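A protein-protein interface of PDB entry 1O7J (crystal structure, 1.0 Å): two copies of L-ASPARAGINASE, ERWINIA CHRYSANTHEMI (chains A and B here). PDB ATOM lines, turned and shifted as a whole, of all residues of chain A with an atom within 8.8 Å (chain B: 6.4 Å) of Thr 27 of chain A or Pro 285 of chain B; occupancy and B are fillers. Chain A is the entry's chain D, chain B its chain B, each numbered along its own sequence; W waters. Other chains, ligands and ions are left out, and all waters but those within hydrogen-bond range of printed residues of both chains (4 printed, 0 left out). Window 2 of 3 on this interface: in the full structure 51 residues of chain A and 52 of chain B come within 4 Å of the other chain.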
ATOM      1  N   THR A  15      -9.193  -1.000  -9.806  1.00  0.00           N
ATOM      2  CA  THR A  15      -8.979  -1.827 -10.986  1.00  0.00           C
ATOM      3  C   THR A  15      -7.862  -2.838 -10.759  1.00  0.00           C
ATOM      4  O   THR A  15      -7.888  -3.947 -11.327  1.00  0.00           O
ATOM      5  CB  THR A  15      -8.726  -0.907 -12.225  1.00  0.00           C
ATOM      6  OG1 THR A  15      -9.969  -0.254 -12.527  1.00  0.00           O
ATOM      7  CG2 THR A  15      -8.210  -1.646 -13.412  1.00  0.00           C
ATOM      8  N   SER A  19     -11.788  -7.611 -11.982  1.00  0.00           N
ATOM      9  CA  SER A  19     -11.941  -8.834 -12.694  1.00  0.00           C
ATOM     10  C   SER A  19     -12.967  -8.688 -13.792  1.00  0.00           C
ATOM     11  O   SER A  19     -14.016  -8.026 -13.607  1.00  0.00           O
ATOM     12  CB  SER A  19     -12.413  -9.842 -11.633  1.00  0.00           C
ATOM     13  OG  SER A  19     -12.156 -11.173 -12.015  1.00  0.00           O
ATOM     14  N   ALA A  20     -12.714  -9.305 -14.937  1.00  0.00           N
ATOM     15  CA  ALA A  20     -13.618  -9.381 -16.073  1.00  0.00           C
ATOM     16  C   ALA A  20     -13.609 -10.838 -16.542  1.00  0.00           C
ATOM     17  O   ALA A  20     -12.701 -11.576 -16.177  1.00  0.00           O
ATOM     18  CB  ALA A  20     -13.269  -8.489 -17.230  1.00  0.00           C
ATOM     19  N   ALA A  21     -14.600 -11.201 -17.365  1.00  0.00           N
ATOM     20  CA  ALA A  21     -14.783 -12.550 -17.812  1.00  0.00           C
ATOM     21  C   ALA A  21     -13.817 -12.986 -18.899  1.00  0.00           C
ATOM     22  O   ALA A  21     -13.711 -14.220 -19.075  1.00  0.00           O
ATOM     23  CB  ALA A  21     -16.219 -12.699 -18.308  1.00  0.00           C
ATOM     24  N   THR A  22     -13.152 -12.058 -19.575  1.00  0.00           N
ATOM     25  CA  THR A  22     -12.172 -12.374 -20.630  1.00  0.00           C
ATOM     26  C   THR A  22     -10.987 -11.453 -20.516  1.00  0.00           C
ATOM     27  O   THR A  22     -11.056 -10.369 -19.923  1.00  0.00           O
ATOM     28  CB  THR A  22     -12.725 -12.225 -22.044  1.00  0.00           C
ATOM     29  OG1 THR A  22     -12.961 -10.823 -22.257  1.00  0.00           O
ATOM     30  CG2 THR A  22     -14.030 -12.992 -22.195  1.00  0.00           C
ATOM     31  N   GLY A  23      -9.862 -11.878 -21.109  1.00  0.00           N
ATOM     32  CA  GLY A  23      -8.641 -11.088 -21.075  1.00  0.00           C
ATOM     33  C   GLY A  23      -8.673  -9.829 -21.886  1.00  0.00           C
ATOM     34  O   GLY A  23      -7.798  -8.965 -21.709  1.00  0.00           O
ATOM     35  N   THR A  24      -9.628  -9.734 -22.820  1.00  0.00           N
ATOM     36  CA  THR A  24      -9.637  -8.579 -23.704  1.00  0.00           C
ATOM     37  C   THR A  24     -10.490  -7.466 -23.126  1.00  0.00           C
ATOM     38  O   THR A  24     -10.510  -6.334 -23.626  1.00  0.00           O
ATOM     39  CB  THR A  24     -10.186  -8.925 -25.117  1.00  0.00           C
ATOM     40  OG1 THR A  24     -11.484  -9.497 -24.970  1.00  0.00           O
ATOM     41  CG2 THR A  24      -9.212  -9.853 -25.857  1.00  0.00           C
ATOM     42  N   GLN A  25     -11.234  -7.736 -22.049  1.00  0.00           N
ATOM     43  CA  GLN A  25     -12.031  -6.641 -21.495  1.00  0.00           C
ATOM     44  C   GLN A  25     -11.221  -5.760 -20.551  1.00  0.00           C
ATOM     45  O   GLN A  25     -10.856  -6.148 -19.456  1.00  0.00           O
ATOM     46  CB  GLN A  25     -13.237  -7.201 -20.731  1.00  0.00           C
ATOM     47  CG  GLN A  25     -14.204  -6.069 -20.415  1.00  0.00           C
ATOM     48  CD  GLN A  25     -15.463  -6.591 -19.766  1.00  0.00           C
ATOM     49  OE1 GLN A  25     -15.822  -7.779 -19.794  1.00  0.00           O
ATOM     50  NE2 GLN A  25     -16.119  -5.602 -19.121  1.00  0.00           N
ATOM     51  N   THR A  26     -10.952  -4.567 -21.058  1.00  0.00           N
ATOM     52  CA  THR A  26     -10.157  -3.591 -20.338  1.00  0.00           C
ATOM     53  C   THR A  26     -10.973  -2.341 -19.995  1.00  0.00           C
ATOM     54  O   THR A  26     -10.434  -1.404 -19.392  1.00  0.00           O
ATOM     55  CB  THR A  26      -8.901  -3.203 -21.095  1.00  0.00           C
ATOM     56  OG1 THR A  26      -9.283  -2.769 -22.399  1.00  0.00           O
ATOM     57  CG2 THR A  26      -7.963  -4.394 -21.272  1.00  0.00           C
ATOM     58  N   THR A  27     -12.214  -2.351 -20.355  1.00  0.00           N
ATOM     59  CA  THR A  27     -13.163  -1.254 -20.026  1.00  0.00           C
ATOM     60  C   THR A  27     -14.438  -1.948 -19.557  1.00  0.00           C
ATOM     61  O   THR A  27     -14.821  -3.081 -19.876  1.00  0.00           O
ATOM     62  CB  THR A  27     -13.403  -0.302 -21.206  1.00  0.00           C
ATOM     63  OG1 THR A  27     -14.017  -1.054 -22.253  1.00  0.00           O
ATOM     64  CG2 THR A  27     -12.120   0.288 -21.761  1.00  0.00           C
ATOM     65  N   GLY A  28     -15.197  -1.276 -18.654  1.00  0.00           N
ATOM     66  CA  GLY A  28     -16.449  -1.847 -18.240  1.00  0.00           C
ATOM     67  C   GLY A  28     -16.484  -2.971 -17.260  1.00  0.00           C
ATOM     68  O   GLY A  28     -17.579  -3.576 -17.062  1.00  0.00           O
ATOM     69  N   TYR A  29     -15.366  -3.315 -16.638  1.00  0.00           N
ATOM     70  CA  TYR A  29     -15.147  -4.451 -15.733  1.00  0.00           C
ATOM     71  C   TYR A  29     -15.531  -4.056 -14.334  1.00  0.00           C
ATOM     72  O   TYR A  29     -15.867  -2.863 -14.032  1.00  0.00           O
ATOM     73  CB  TYR A  29     -13.674  -5.008 -15.782  1.00  0.00           C
ATOM     74  CG  TYR A  29     -12.820  -3.774 -15.575  1.00  0.00           C
ATOM     75  CD1 TYR A  29     -12.559  -3.356 -14.296  1.00  0.00           C
ATOM     76  CD2 TYR A  29     -12.316  -3.077 -16.668  1.00  0.00           C
ATOM     77  CE1 TYR A  29     -11.760  -2.232 -14.154  1.00  0.00           C
ATOM     78  CE2 TYR A  29     -11.542  -1.916 -16.511  1.00  0.00           C
ATOM     79  CZ  TYR A  29     -11.281  -1.512 -15.207  1.00  0.00           C
ATOM     80  OH  TYR A  29     -10.569  -0.362 -15.071  1.00  0.00           O
ATOM     81  N   LYS A  30     -15.478  -4.989 -13.410  1.00  0.00           N
ATOM     82  CA  LYS A  30     -15.744  -4.777 -11.984  1.00  0.00           C
ATOM     83  C   LYS A  30     -14.509  -4.438 -11.184  1.00  0.00           C
ATOM     84  O   LYS A  30     -13.673  -5.311 -10.941  1.00  0.00           O
ATOM     85  CB  LYS A  30     -16.412  -6.035 -11.416  1.00  0.00           C
ATOM     86  CG  LYS A  30     -16.900  -5.935  -9.974  1.00  0.00           C
ATOM     87  N   MET A 121      -4.114   0.330 -14.300  1.00  0.00           N
ATOM     88  CA  MET A 121      -5.026   0.796 -15.344  1.00  0.00           C
ATOM     89  C   MET A 121      -5.759  -0.321 -16.087  1.00  0.00           C
ATOM     90  O   MET A 121      -6.786  -0.030 -16.697  1.00  0.00           O
ATOM     91  CB  MET A 121      -4.289   1.707 -16.324  1.00  0.00           C
ATOM     92  CG  MET A 121      -3.982   3.079 -15.732  1.00  0.00           C
ATOM     93  SD  MET A 121      -5.498   4.055 -15.441  1.00  0.00           S
ATOM     94  CE  MET A 121      -5.931   4.523 -17.116  1.00  0.00           C
ATOM     95  N   ARG A 122      -5.266  -1.551 -16.004  1.00  0.00           N
ATOM     96  CA  ARG A 122      -5.930  -2.734 -16.566  1.00  0.00           C
ATOM     97  C   ARG A 122      -6.317  -3.647 -15.402  1.00  0.00           C
ATOM     98  O   ARG A 122      -5.592  -3.760 -14.420  1.00  0.00           O
ATOM     99  CB  ARG A 122      -5.032  -3.462 -17.528  1.00  0.00           C
ATOM    100  CG  ARG A 122      -4.722  -2.708 -18.796  1.00  0.00           C
ATOM    101  CD  ARG A 122      -3.671  -3.392 -19.642  1.00  0.00           C
ATOM    102  NE  ARG A 122      -3.378  -2.620 -20.846  1.00  0.00           N
ATOM    103  CZ  ARG A 122      -2.288  -2.769 -21.601  1.00  0.00           C
ATOM    104  NH1 ARG A 122      -1.395  -3.702 -21.305  1.00  0.00           N
ATOM    105  NH2 ARG A 122      -2.102  -1.974 -22.639  1.00  0.00           N
ATOM    106  N   PRO A 123      -7.484  -4.328 -15.507  1.00  0.00           N
ATOM    107  CA  PRO A 123      -7.852  -5.268 -14.430  1.00  0.00           C
ATOM    108  C   PRO A 123      -6.916  -6.436 -14.356  1.00  0.00           C
ATOM    109  O   PRO A 123      -6.179  -6.750 -15.273  1.00  0.00           O
ATOM    110  CB  PRO A 123      -9.300  -5.658 -14.835  1.00  0.00           C
ATOM    111  CG  PRO A 123      -9.311  -5.528 -16.346  1.00  0.00           C
ATOM    112  CD  PRO A 123      -8.445  -4.302 -16.608  1.00  0.00           C
ATOM    113  N   ALA A 126      -6.715  -8.941 -17.248  1.00  0.00           N
ATOM    114  CA  ALA A 126      -6.433  -8.484 -18.606  1.00  0.00           C
ATOM    115  C   ALA A 126      -5.151  -9.094 -19.146  1.00  0.00           C
ATOM    116  O   ALA A 126      -4.176  -9.352 -18.437  1.00  0.00           O
ATOM    117  CB  ALA A 126      -6.232  -6.955 -18.615  1.00  0.00           C
ATOM    118  N   ASN A 170      -4.528  11.105 -18.189  1.00  0.00           N
ATOM    119  CA  ASN A 170      -5.194  10.486 -19.332  1.00  0.00           C
ATOM    120  C   ASN A 170      -6.278   9.530 -18.811  1.00  0.00           C
ATOM    121  O   ASN A 170      -6.098   8.799 -17.839  1.00  0.00           O
ATOM    122  CB  ASN A 170      -4.159   9.757 -20.178  1.00  0.00           C
ATOM    123  CG  ASN A 170      -4.676   9.258 -21.526  1.00  0.00           C
ATOM    124  OD1 ASN A 170      -5.573   8.400 -21.583  1.00  0.00           O
ATOM    125  ND2 ASN A 170      -4.109   9.790 -22.604  1.00  0.00           N
ATOM    126  N   ALA A 171      -7.421   9.559 -19.491  1.00  0.00           N
ATOM    127  CA  ALA A 171      -8.532   8.714 -19.081  1.00  0.00           C
ATOM    128  C   ALA A 171      -8.162   7.226 -19.030  1.00  0.00           C
ATOM    129  O   ALA A 171      -8.758   6.527 -18.210  1.00  0.00           O
ATOM    130  CB  ALA A 171      -9.679   8.939 -20.060  1.00  0.00           C
ATOM    131  N   SER A 172      -7.309   6.750 -19.941  1.00  0.00           N
ATOM    132  CA  SER A 172      -7.292   5.317 -20.270  1.00  0.00           C
ATOM    133  C   SER A 172      -5.925   4.645 -20.459  1.00  0.00           C
ATOM    134  O   SER A 172      -5.918   3.425 -20.625  1.00  0.00           O
ATOM    135  CB  SER A 172      -8.177   5.099 -21.508  1.00  0.00           C
ATOM    136  OG  SER A 172      -9.503   5.409 -21.216  1.00  0.00           O
ATOM    137  N   ALA B 252     -11.917   7.716 -16.636  1.00  0.00           N
ATOM    138  CA  ALA B 252     -12.563   7.546 -17.921  1.00  0.00           C
ATOM    139  C   ALA B 252     -14.063   7.746 -17.801  1.00  0.00           C
ATOM    140  O   ALA B 252     -14.900   6.883 -18.065  1.00  0.00           O
ATOM    141  CB  ALA B 252     -12.227   6.153 -18.485  1.00  0.00           C
ATOM    142  N   GLY B 253     -14.452   8.954 -17.374  1.00  0.00           N
ATOM    143  CA  GLY B 253     -15.856   9.290 -17.211  1.00  0.00           C
ATOM    144  C   GLY B 253     -16.538   8.520 -16.110  1.00  0.00           C
ATOM    145  O   GLY B 253     -17.779   8.380 -16.156  1.00  0.00           O
ATOM    146  N   ARG B 275     -20.547  12.216 -20.769  1.00  0.00           N
ATOM    147  CA  ARG B 275     -19.437  11.910 -19.854  1.00  0.00           C
ATOM    148  C   ARG B 275     -18.102  12.160 -20.552  1.00  0.00           C
ATOM    149  O   ARG B 275     -17.726  11.429 -21.485  1.00  0.00           O
ATOM    150  CB  ARG B 275     -19.533  10.482 -19.337  1.00  0.00           C
ATOM    151  CG  ARG B 275     -20.826  10.203 -18.594  1.00  0.00           C
ATOM    152  CD  ARG B 275     -20.872   8.889 -17.812  1.00  0.00           C
ATOM    153  NE  ARG B 275     -20.902   7.684 -18.664  1.00  0.00           N
ATOM    154  CZ  ARG B 275     -19.872   6.948 -19.024  1.00  0.00           C
ATOM    155  NH1 ARG B 275     -18.638   7.211 -18.614  1.00  0.00           N
ATOM    156  NH2 ARG B 275     -20.034   5.902 -19.806  1.00  0.00           N
ATOM    157  N   ILE B 283      -9.199   8.945 -24.129  1.00  0.00           N
ATOM    158  CA  ILE B 283     -10.497   8.433 -24.546  1.00  0.00           C
ATOM    159  C   ILE B 283     -11.378   8.059 -23.385  1.00  0.00           C
ATOM    160  O   ILE B 283     -10.992   7.245 -22.538  1.00  0.00           O
ATOM    161  CB  ILE B 283     -10.290   7.149 -25.421  1.00  0.00           C
ATOM    162  CG1 ILE B 283      -9.485   7.404 -26.664  1.00  0.00           C
ATOM    163  CG2 ILE B 283     -11.640   6.513 -25.753  1.00  0.00           C
ATOM    164  CD1 ILE B 283     -10.121   8.361 -27.634  1.00  0.00           C
ATOM    165  N   VAL B 284     -12.613   8.585 -23.404  1.00  0.00           N
ATOM    166  CA  VAL B 284     -13.683   8.079 -22.530  1.00  0.00           C
ATOM    167  C   VAL B 284     -14.423   7.021 -23.380  1.00  0.00           C
ATOM    168  O   VAL B 284     -15.090   7.410 -24.369  1.00  0.00           O
ATOM    169  CB  VAL B 284     -14.622   9.161 -22.034  1.00  0.00           C
ATOM    170  CG1 VAL B 284     -15.729   8.527 -21.198  1.00  0.00           C
ATOM    171  CG2 VAL B 284     -13.855  10.186 -21.225  1.00  0.00           C
ATOM    172  N   PRO B 285     -14.272   5.728 -23.059  1.00  0.00           N
ATOM    173  CA  PRO B 285     -14.824   4.639 -23.910  1.00  0.00           C
ATOM    174  C   PRO B 285     -16.271   4.406 -23.616  1.00  0.00           C
ATOM    175  O   PRO B 285     -16.761   4.718 -22.529  1.00  0.00           O
ATOM    176  CB  PRO B 285     -13.998   3.438 -23.487  1.00  0.00           C
ATOM    177  CG  PRO B 285     -13.788   3.668 -22.000  1.00  0.00           C
ATOM    178  CD  PRO B 285     -13.616   5.161 -21.862  1.00  0.00           C
ATOM    179  N   PRO B 286     -17.014   3.800 -24.546  1.00  0.00           N
ATOM    180  CA  PRO B 286     -18.397   3.405 -24.236  1.00  0.00           C
ATOM    181  C   PRO B 286     -18.455   2.452 -23.067  1.00  0.00           C
ATOM    182  O   PRO B 286     -17.567   1.620 -22.835  1.00  0.00           O
ATOM    183  CB  PRO B 286     -18.878   2.741 -25.554  1.00  0.00           C
ATOM    184  CG  PRO B 286     -17.836   2.905 -26.568  1.00  0.00           C
ATOM    185  CD  PRO B 286     -16.598   3.403 -25.902  1.00  0.00           C
ATOM    186  N   ASP B 287     -19.578   2.484 -22.337  1.00  0.00           N
ATOM    187  CA  ASP B 287     -19.799   1.559 -21.250  1.00  0.00           C
ATOM    188  C   ASP B 287     -21.315   1.489 -21.013  1.00  0.00           C
ATOM    189  O   ASP B 287     -21.880   2.430 -20.420  1.00  0.00           O
ATOM    190  CB  ASP B 287     -19.092   1.956 -19.972  1.00  0.00           C
ATOM    191  CG  ASP B 287     -19.292   0.979 -18.834  1.00  0.00           C
ATOM    192  OD1 ASP B 287     -20.119   0.055 -18.911  1.00  0.00           O
ATOM    193  OD2 ASP B 287     -18.560   1.137 -17.820  1.00  0.00           O
ATOM    194  N   VAL B 294     -20.708   9.215 -24.143  1.00  0.00           N
ATOM    195  CA  VAL B 294     -19.259   9.341 -23.858  1.00  0.00           C
ATOM    196  C   VAL B 294     -18.612  10.311 -24.841  1.00  0.00           C
ATOM    197  O   VAL B 294     -19.008  10.440 -26.027  1.00  0.00           O
ATOM    198  CB  VAL B 294     -18.535   7.993 -23.845  1.00  0.00           C
ATOM    199  CG1 VAL B 294     -19.100   7.107 -22.717  1.00  0.00           C
ATOM    200  CG2 VAL B 294     -18.538   7.275 -25.194  1.00  0.00           C
ATOM    201  N   SER B 295     -17.566  10.982 -24.365  1.00  0.00           N
ATOM    202  CA  SER B 295     -17.020  12.131 -25.122  1.00  0.00           C
ATOM    203  C   SER B 295     -15.862  11.769 -26.074  1.00  0.00           C
ATOM    204  O   SER B 295     -15.317  12.731 -26.640  1.00  0.00           O
ATOM    205  CB  SER B 295     -16.599  13.267 -24.214  1.00  0.00           C
ATOM    206  OG  SER B 295     -15.411  12.980 -23.526  1.00  0.00           O
ATOM    207  N   ASP B 296     -15.530  10.506 -26.236  1.00  0.00           N
ATOM    208  CA  ASP B 296     -14.396  10.172 -27.128  1.00  0.00           C
ATOM    209  C   ASP B 296     -13.182  10.914 -26.547  1.00  0.00           C
ATOM    210  O   ASP B 296     -12.994  10.854 -25.317  1.00  0.00           O
ATOM    211  CB  ASP B 296     -14.813  10.479 -28.586  1.00  0.00           C
ATOM    212  CG  ASP B 296     -13.933   9.992 -29.688  1.00  0.00           C
ATOM    213  OD1 ASP B 296     -12.789  10.474 -29.841  1.00  0.00           O
ATOM    214  OD2 ASP B 296     -14.394   9.075 -30.477  1.00  0.00           O
HETATM  215  O   HOH W   1      -6.718   7.346 -23.940  1.00  0.00           O
HETATM  216  O   HOH W   2     -19.553  -2.558 -18.874  1.00  0.00           O
HETATM  217  O   HOH W   3     -16.849  -0.618 -21.344  1.00  0.00           O
HETATM  218  O   HOH W   4     -15.562   0.181 -23.988  1.00  0.00           O
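The backbone carbonyl oxygen of Ile 283 of chain B lies within hydrogen-bond range of the side-chain hydroxyl of Ser 172 of chain A.
NE2 of Gln 25 of chain A sits at hydrogen-bond distance from O of Gly 28 of chain A (3.2 Å). N of Ser 172 of chain A is in hydrogen-bond range of OD1 of Asn 170 of chain A (2.9 Å). NE2 of Gln 25 of chain A is in hydrogen-bond range of O of Thr 27 of chain A, 2.9 Å away.
Among the printed residues, pairs that only touch across the chains: Thr 27 of chain A with Pro 285 of chain B, Gly 28 of chain A with Asp 287 of chain B, Ala 171 of chain A with Ala 252 of chain B, Ala 171 of chain A with Ile 283 of chain B and Ser 172 of chain A with Ala 252 of chain B.
Of chain B, only Pro 285 comes within 4 Å of Thr 27 of chain A. Of the printed residues of chain B, Gly 28 of chain A touches Asp 287. Printed residues of chain B within 4 Å of Ala 171 of chain A: Ala 252 and Ile 283. Printed residues of chain B within 4 Å of Ser 172 of chain A: Ala 252 (3.9 Å) and Ile 283 (2.7 Å). Of the printed residues of chain A, Ile 283 of chain B touches Ala 171 (3.3 Å) and Ser 172 (2.7 Å). Printed residues of chain A within 4 Å of Pro 285 of chain B: Thr 27. No residue of chain A comes within 4 Å of Pro 286 of chain B. Printed residues of chain A within 4 Å of Asp 287 of chain B: Gly 28 (3.7 Å).
Of the 11 printed residues of chain B, 4 touch a printed residue of chain A. Printed residues of chain B that touch a printed residue of chain A: Ala 252, Ile 283, Pro 285 and Asp 287. Among the printed residues, 6 pairs touch across the chains. Among the printed residues, no Asp or Glu carboxylate lies within 4 Å of a Lys or Arg side-chain nitrogen of the other chain.
No position is printed for both chains. Of the 6 pairs that touch across the chains among the printed residues, none has its exchanged pair printed and touching as well.
Water W4 lies within hydrogen-bond range of the side-chain hydroxyl of Thr 27 of chain A and the backbone carbonyl oxygen of Pro 286 of chain B. Water W2 lies within hydrogen-bond range of OD1 of Asp 287 of chain B and O of Gly 28 of chain A. Water W3 lies within hydrogen-bond range of the backbone carbonyl oxygen (O) of Pro 286 of chain B (2.8 Å), the side-chain hydroxyl (OG1) of Thr 27 of chain A (3.0 Å) and the backbone NH (N) of Gly 28 of chain A (3.2 Å). Water W1 lies within hydrogen-bond range of OD1 of Asn 170 of chain A (2.8 Å) and N of Ile 283 of chain B (3.0 Å).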
